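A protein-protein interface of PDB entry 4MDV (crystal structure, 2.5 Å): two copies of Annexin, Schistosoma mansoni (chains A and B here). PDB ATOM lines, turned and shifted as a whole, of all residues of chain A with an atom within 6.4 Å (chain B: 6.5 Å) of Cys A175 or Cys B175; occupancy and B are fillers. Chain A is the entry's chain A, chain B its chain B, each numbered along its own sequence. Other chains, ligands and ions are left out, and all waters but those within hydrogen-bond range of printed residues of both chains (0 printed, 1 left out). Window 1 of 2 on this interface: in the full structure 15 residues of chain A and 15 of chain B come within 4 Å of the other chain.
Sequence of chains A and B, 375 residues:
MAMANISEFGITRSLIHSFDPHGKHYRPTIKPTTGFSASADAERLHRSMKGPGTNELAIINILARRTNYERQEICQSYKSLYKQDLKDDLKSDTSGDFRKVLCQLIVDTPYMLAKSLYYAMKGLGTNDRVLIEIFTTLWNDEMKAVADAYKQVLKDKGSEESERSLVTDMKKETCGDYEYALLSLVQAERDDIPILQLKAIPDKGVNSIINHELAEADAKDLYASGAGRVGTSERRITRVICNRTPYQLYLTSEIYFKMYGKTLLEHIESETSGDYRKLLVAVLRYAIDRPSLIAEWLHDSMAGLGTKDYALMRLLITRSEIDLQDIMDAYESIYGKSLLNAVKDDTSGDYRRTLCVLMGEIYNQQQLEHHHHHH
Of the printed residues of chain B, Thr A174 touches Cys B175 (3.7 Å).
Cys A175 touches just these residues of chain B: Thr B174 (3.7 Å) and Cys B175 (2.1 Å).
Gly A176 touches none of the printed residues of chain B.
Of the printed residues of chain A, Thr B174 touches Cys A175.
Cys B175 touches two residues of chain A.
Asp B177 touches none of the printed residues of chain A.
The nearest residue of chain B that does not touch Cys A175 is Glu B173 (4.4 Å).
The nearest printed residue of chain A that does not touch Thr B174 is Gly A176 (6.6 Å).
The backbone carbonyl oxygen (O) of Met B170 sits at hydrogen-bond distance from the side-chain hydroxyl (OG1) of Thr B174.
Of the 11 printed residues of chain A, 2 touch a printed residue of chain B.
Printed residues of chain A that touch a printed residue of chain B: Thr A174 and Cys A175.
Among the printed residues, 3 pairs touch across the chains.
Among the printed residues, no Asp or Glu carboxylate lies within 4 Å of a Lys or Arg side-chain nitrogen of the other chain.
SG of Cys A175 is disulfide-bonded to SG of Cys B175, at 2.1 Å.
Among the printed residues, merely in contact across the chains: Thr A174 with Cys B175 (3.7 Å) and Cys A175 with Thr B174 (3.7 Å).
Thr A174 touches Cys B175, and with the chains exchanged Cys A175 touches Thr B174.
Cys B175 touches its own counterpart, Cys A175.
Positions printed for both chains: 170, 171, 172, 173, 174, 175, 176, 177, 178, 179 and 180.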
ATOM      1  N   MET A 170      -1.867  21.628  -5.460  1.00  0.00           N
ATOM      2  CA  MET A 170      -2.786  22.002  -4.386  1.00  0.00           C
ATOM      3  C   MET A 170      -2.937  23.505  -4.224  1.00  0.00           C
ATOM      4  O   MET A 170      -4.052  24.005  -4.095  1.00  0.00           O
ATOM      5  CB  MET A 170      -2.330  21.452  -3.045  1.00  0.00           C
ATOM      6  CG  MET A 170      -2.335  19.976  -2.911  1.00  0.00           C
ATOM      7  SD  MET A 170      -1.759  19.625  -1.261  1.00  0.00           S
ATOM      8  CE  MET A 170      -2.987  20.498  -0.293  1.00  0.00           C
ATOM      9  N   LYS A 171      -1.814  24.218  -4.184  1.00  0.00           N
ATOM     10  CA  LYS A 171      -1.839  25.667  -4.024  1.00  0.00           C
ATOM     11  C   LYS A 171      -2.786  26.298  -5.046  1.00  0.00           C
ATOM     12  O   LYS A 171      -3.627  27.141  -4.698  1.00  0.00           O
ATOM     13  CB  LYS A 171      -0.432  26.248  -4.187  1.00  0.00           C
ATOM     14  CG  LYS A 171      -0.394  27.774  -4.181  1.00  0.00           C
ATOM     15  CD  LYS A 171       0.874  28.325  -4.843  1.00  0.00           C
ATOM     16  CE  LYS A 171       0.689  29.787  -5.274  1.00  0.00           C
ATOM     17  NZ  LYS A 171       1.941  30.436  -5.772  1.00  0.00           N
ATOM     18  N   LYS A 172      -2.638  25.886  -6.307  1.00  0.00           N
ATOM     19  CA  LYS A 172      -3.477  26.390  -7.394  1.00  0.00           C
ATOM     20  C   LYS A 172      -4.921  25.945  -7.193  1.00  0.00           C
ATOM     21  O   LYS A 172      -5.868  26.644  -7.565  1.00  0.00           O
ATOM     22  CB  LYS A 172      -2.956  25.914  -8.752  1.00  0.00           C
ATOM     23  N   GLU A 173      -5.065  24.782  -6.570  1.00  0.00           N
ATOM     24  CA  GLU A 173      -6.343  24.105  -6.412  1.00  0.00           C
ATOM     25  C   GLU A 173      -7.122  24.613  -5.198  1.00  0.00           C
ATOM     26  O   GLU A 173      -8.344  24.464  -5.120  1.00  0.00           O
ATOM     27  CB  GLU A 173      -6.053  22.614  -6.245  1.00  0.00           C
ATOM     28  CG  GLU A 173      -7.196  21.717  -6.581  1.00  0.00           C
ATOM     29  CD  GLU A 173      -7.567  21.795  -8.038  1.00  0.00           C
ATOM     30  OE1 GLU A 173      -6.709  22.204  -8.842  1.00  0.00           O
ATOM     31  OE2 GLU A 173      -8.716  21.454  -8.372  1.00  0.00           O
ATOM     32  N   THR A 174      -6.404  25.228  -4.263  1.00  0.00           N
ATOM     33  CA  THR A 174      -6.960  25.474  -2.938  1.00  0.00           C
ATOM     34  C   THR A 174      -6.642  26.869  -2.355  1.00  0.00           C
ATOM     35  O   THR A 174      -5.736  27.570  -2.828  1.00  0.00           O
ATOM     36  CB  THR A 174      -6.537  24.338  -1.987  1.00  0.00           C
ATOM     37  OG1 THR A 174      -7.414  24.298  -0.858  1.00  0.00           O
ATOM     38  CG2 THR A 174      -5.092  24.520  -1.543  1.00  0.00           C
ATOM     39  N   CYS A 175      -7.408  27.263  -1.339  1.00  0.00           N
ATOM     40  CA  CYS A 175      -7.326  28.611  -0.768  1.00  0.00           C
ATOM     41  C   CYS A 175      -7.850  28.648   0.671  1.00  0.00           C
ATOM     42  O   CYS A 175      -8.450  27.666   1.140  1.00  0.00           O
ATOM     43  CB  CYS A 175      -8.125  29.599  -1.621  1.00  0.00           C
ATOM     44  SG  CYS A 175      -9.872  29.152  -1.808  1.00  0.00           S
ATOM     45  N   GLY A 176      -7.621  29.784   1.345  1.00  0.00           N
ATOM     46  CA  GLY A 176      -8.127  30.044   2.685  1.00  0.00           C
ATOM     47  C   GLY A 176      -7.584  29.166   3.814  1.00  0.00           C
ATOM     48  O   GLY A 176      -6.492  28.591   3.706  1.00  0.00           O
ATOM     49  N   ASP A 177      -8.366  29.059   4.894  1.00  0.00           N
ATOM     50  CA  ASP A 177      -8.016  28.247   6.077  1.00  0.00           C
ATOM     51  C   ASP A 177      -7.725  26.802   5.710  1.00  0.00           C
ATOM     52  O   ASP A 177      -6.757  26.175   6.193  1.00  0.00           O
ATOM     53  CB  ASP A 177      -9.176  28.262   7.087  1.00  0.00           C
ATOM     54  CG  ASP A 177      -9.410  29.642   7.695  1.00  0.00           C
ATOM     55  OD1 ASP A 177      -8.428  30.395   7.885  1.00  0.00           O
ATOM     56  OD2 ASP A 177     -10.571  29.979   7.993  1.00  0.00           O
ATOM     57  N   TYR A 178      -8.606  26.288   4.859  1.00  0.00           N
ATOM     58  CA  TYR A 178      -8.523  24.947   4.313  1.00  0.00           C
ATOM     59  C   TYR A 178      -7.193  24.697   3.576  1.00  0.00           C
ATOM     60  O   TYR A 178      -6.554  23.653   3.770  1.00  0.00           O
ATOM     61  CB  TYR A 178      -9.767  24.737   3.437  1.00  0.00           C
ATOM     62  CG  TYR A 178      -9.855  23.436   2.704  1.00  0.00           C
ATOM     63  CD1 TYR A 178      -9.896  22.226   3.382  1.00  0.00           C
ATOM     64  CD2 TYR A 178      -9.934  23.423   1.312  1.00  0.00           C
ATOM     65  CE1 TYR A 178      -9.973  21.016   2.675  1.00  0.00           C
ATOM     66  CE2 TYR A 178     -10.024  22.238   0.602  1.00  0.00           C
ATOM     67  CZ  TYR A 178     -10.038  21.038   1.276  1.00  0.00           C
ATOM     68  OH  TYR A 178     -10.104  19.880   0.529  1.00  0.00           O
ATOM     69  N   GLU A 179      -6.752  25.665   2.776  1.00  0.00           N
ATOM     70  CA  GLU A 179      -5.490  25.524   2.055  1.00  0.00           C
ATOM     71  C   GLU A 179      -4.339  25.429   3.032  1.00  0.00           C
ATOM     72  O   GLU A 179      -3.484  24.547   2.938  1.00  0.00           O
ATOM     73  CB  GLU A 179      -5.277  26.717   1.140  1.00  0.00           C
ATOM     74  CG  GLU A 179      -3.849  26.875   0.635  1.00  0.00           C
ATOM     75  CD  GLU A 179      -3.667  28.165  -0.144  1.00  0.00           C
ATOM     76  OE1 GLU A 179      -3.667  28.087  -1.396  1.00  0.00           O
ATOM     77  OE2 GLU A 179      -3.542  29.246   0.491  1.00  0.00           O
ATOM     78  N   TYR A 180      -4.331  26.356   3.975  1.00  0.00           N
ATOM     79  CA  TYR A 180      -3.274  26.428   4.951  1.00  0.00           C
ATOM     80  C   TYR A 180      -3.153  25.089   5.686  1.00  0.00           C
ATOM     81  O   TYR A 180      -2.050  24.542   5.847  1.00  0.00           O
ATOM     82  CB  TYR A 180      -3.565  27.563   5.931  1.00  0.00           C
ATOM     83  CG  TYR A 180      -2.404  27.835   6.847  1.00  0.00           C
ATOM     84  CD1 TYR A 180      -2.193  27.050   7.985  1.00  0.00           C
ATOM     85  CD2 TYR A 180      -1.502  28.867   6.574  1.00  0.00           C
ATOM     86  CE1 TYR A 180      -1.120  27.285   8.835  1.00  0.00           C
ATOM     87  CE2 TYR A 180      -0.431  29.121   7.423  1.00  0.00           C
ATOM     88  CZ  TYR A 180      -0.240  28.325   8.553  1.00  0.00           C
ATOM     89  OH  TYR A 180       0.831  28.568   9.395  1.00  0.00           O
ATOM     90  N   MET B 170     -15.984  37.625  -0.912  1.00  0.00           N
ATOM     91  CA  MET B 170     -16.008  36.330  -1.602  1.00  0.00           C
ATOM     92  C   MET B 170     -14.671  35.965  -2.228  1.00  0.00           C
ATOM     93  O   MET B 170     -14.191  34.842  -2.082  1.00  0.00           O
ATOM     94  CB  MET B 170     -17.077  36.307  -2.684  1.00  0.00           C
ATOM     95  CG  MET B 170     -18.467  36.270  -2.168  1.00  0.00           C
ATOM     96  SD  MET B 170     -19.590  36.352  -3.551  1.00  0.00           S
ATOM     97  CE  MET B 170     -19.169  34.807  -4.354  1.00  0.00           C
ATOM     98  N   LYS B 171     -14.079  36.910  -2.947  1.00  0.00           N
ATOM     99  CA  LYS B 171     -12.797  36.649  -3.588  1.00  0.00           C
ATOM    100  C   LYS B 171     -11.782  36.155  -2.559  1.00  0.00           C
ATOM    101  O   LYS B 171     -11.075  35.178  -2.803  1.00  0.00           O
ATOM    102  CB  LYS B 171     -12.282  37.876  -4.356  1.00  0.00           C
ATOM    103  CG  LYS B 171     -13.110  38.239  -5.601  1.00  0.00           C
ATOM    104  CD  LYS B 171     -12.301  39.088  -6.600  1.00  0.00           C
ATOM    105  CE  LYS B 171     -13.155  39.542  -7.794  1.00  0.00           C
ATOM    106  NZ  LYS B 171     -12.368  39.930  -9.015  1.00  0.00           N
ATOM    107  N   LYS B 172     -11.730  36.813  -1.404  1.00  0.00           N
ATOM    108  CA  LYS B 172     -10.818  36.402  -0.334  1.00  0.00           C
ATOM    109  C   LYS B 172     -11.209  35.014   0.170  1.00  0.00           C
ATOM    110  O   LYS B 172     -10.355  34.211   0.564  1.00  0.00           O
ATOM    111  CB  LYS B 172     -10.833  37.414   0.829  1.00  0.00           C
ATOM    112  N   GLU B 173     -12.509  34.736   0.138  1.00  0.00           N
ATOM    113  CA  GLU B 173     -13.060  33.536   0.756  1.00  0.00           C
ATOM    114  C   GLU B 173     -13.034  32.344  -0.198  1.00  0.00           C
ATOM    115  O   GLU B 173     -13.161  31.185   0.226  1.00  0.00           O
ATOM    116  CB  GLU B 173     -14.484  33.808   1.248  1.00  0.00           C
ATOM    117  CG  GLU B 173     -15.072  32.759   2.201  1.00  0.00           C
ATOM    118  CD  GLU B 173     -14.656  32.898   3.691  1.00  0.00           C
ATOM    119  OE1 GLU B 173     -13.707  33.639   4.037  1.00  0.00           O
ATOM    120  OE2 GLU B 173     -15.290  32.231   4.541  1.00  0.00           O
ATOM    121  N   THR B 174     -12.813  32.632  -1.482  1.00  0.00           N
ATOM    122  CA  THR B 174     -13.085  31.668  -2.543  1.00  0.00           C
ATOM    123  C   THR B 174     -12.002  31.570  -3.624  1.00  0.00           C
ATOM    124  O   THR B 174     -11.237  32.510  -3.832  1.00  0.00           O
ATOM    125  CB  THR B 174     -14.419  32.017  -3.229  1.00  0.00           C
ATOM    126  OG1 THR B 174     -15.447  32.160  -2.236  1.00  0.00           O
ATOM    127  CG2 THR B 174     -14.809  30.936  -4.191  1.00  0.00           C
ATOM    128  N   CYS B 175     -11.955  30.428  -4.316  1.00  0.00           N
ATOM    129  CA  CYS B 175     -10.922  30.154  -5.329  1.00  0.00           C
ATOM    130  C   CYS B 175     -11.397  29.145  -6.366  1.00  0.00           C
ATOM    131  O   CYS B 175     -12.456  28.514  -6.201  1.00  0.00           O
ATOM    132  CB  CYS B 175      -9.620  29.622  -4.702  1.00  0.00           C
ATOM    133  SG  CYS B 175      -9.842  28.167  -3.607  1.00  0.00           S
ATOM    134  N   GLY B 176     -10.601  29.004  -7.429  1.00  0.00           N
ATOM    135  CA  GLY B 176     -10.827  27.990  -8.443  1.00  0.00           C
ATOM    136  C   GLY B 176     -12.076  28.157  -9.300  1.00  0.00           C
ATOM    137  O   GLY B 176     -12.626  29.256  -9.449  1.00  0.00           O
ATOM    138  N   ASP B 177     -12.527  27.045  -9.873  1.00  0.00           N
ATOM    139  CA  ASP B 177     -13.712  27.050 -10.721  1.00  0.00           C
ATOM    140  C   ASP B 177     -14.961  27.521  -9.970  1.00  0.00           C
ATOM    141  O   ASP B 177     -15.766  28.295 -10.499  1.00  0.00           O
ATOM    142  CB  ASP B 177     -13.870  25.685 -11.390  1.00  0.00           C
ATOM    143  CG  ASP B 177     -12.700  25.377 -12.316  1.00  0.00           C
ATOM    144  OD1 ASP B 177     -12.260  26.341 -12.983  1.00  0.00           O
ATOM    145  OD2 ASP B 177     -12.203  24.216 -12.349  1.00  0.00           O
ATOM    146  N   TYR B 178     -15.083  27.080  -8.721  1.00  0.00           N
ATOM    147  CA  TYR B 178     -16.132  27.512  -7.811  1.00  0.00           C
ATOM    148  C   TYR B 178     -16.163  29.037  -7.667  1.00  0.00           C
ATOM    149  O   TYR B 178     -17.230  29.659  -7.736  1.00  0.00           O
ATOM    150  CB  TYR B 178     -15.860  26.897  -6.439  1.00  0.00           C
ATOM    151  CG  TYR B 178     -16.822  27.276  -5.334  1.00  0.00           C
ATOM    152  CD1 TYR B 178     -18.201  27.108  -5.487  1.00  0.00           C
ATOM    153  CD2 TYR B 178     -16.355  27.750  -4.115  1.00  0.00           C
ATOM    154  CE1 TYR B 178     -19.087  27.425  -4.462  1.00  0.00           C
ATOM    155  CE2 TYR B 178     -17.240  28.066  -3.073  1.00  0.00           C
ATOM    156  CZ  TYR B 178     -18.601  27.894  -3.258  1.00  0.00           C
ATOM    157  OH  TYR B 178     -19.474  28.194  -2.251  1.00  0.00           O
ATOM    158  N   GLU B 179     -14.997  29.644  -7.438  1.00  0.00           N
ATOM    159  CA  GLU B 179     -14.949  31.095  -7.261  1.00  0.00           C
ATOM    160  C   GLU B 179     -15.480  31.770  -8.504  1.00  0.00           C
ATOM    161  O   GLU B 179     -16.303  32.688  -8.434  1.00  0.00           O
ATOM    162  CB  GLU B 179     -13.526  31.608  -6.982  1.00  0.00           C
ATOM    163  CG  GLU B 179     -13.312  33.122  -7.288  1.00  0.00           C
ATOM    164  CD  GLU B 179     -12.018  33.716  -6.678  1.00  0.00           C
ATOM    165  OE1 GLU B 179     -12.090  34.816  -6.090  1.00  0.00           O
ATOM    166  OE2 GLU B 179     -10.928  33.108  -6.776  1.00  0.00           O
ATOM    167  N   TYR B 180     -14.987  31.313  -9.651  1.00  0.00           N
ATOM    168  CA  TYR B 180     -15.318  31.952 -10.895  1.00  0.00           C
ATOM    169  C   TYR B 180     -16.825  31.903 -11.119  1.00  0.00           C
ATOM    170  O   TYR B 180     -17.435  32.913 -11.490  1.00  0.00           O
ATOM    171  CB  TYR B 180     -14.552  31.292 -12.039  1.00  0.00           C
ATOM    172  CG  TYR B 180     -14.843  31.916 -13.374  1.00  0.00           C
ATOM    173  CD1 TYR B 180     -15.911  31.469 -14.148  1.00  0.00           C
ATOM    174  CD2 TYR B 180     -14.056  32.958 -13.862  1.00  0.00           C
ATOM    175  CE1 TYR B 180     -16.186  32.039 -15.375  1.00  0.00           C
ATOM    176  CE2 TYR B 180     -14.326  33.539 -15.093  1.00  0.00           C
ATOM    177  CZ  TYR B 180     -15.394  33.072 -15.842  1.00  0.00           C
ATOM    178  OH  TYR B 180     -15.677  33.627 -17.067  1.00  0.00           O
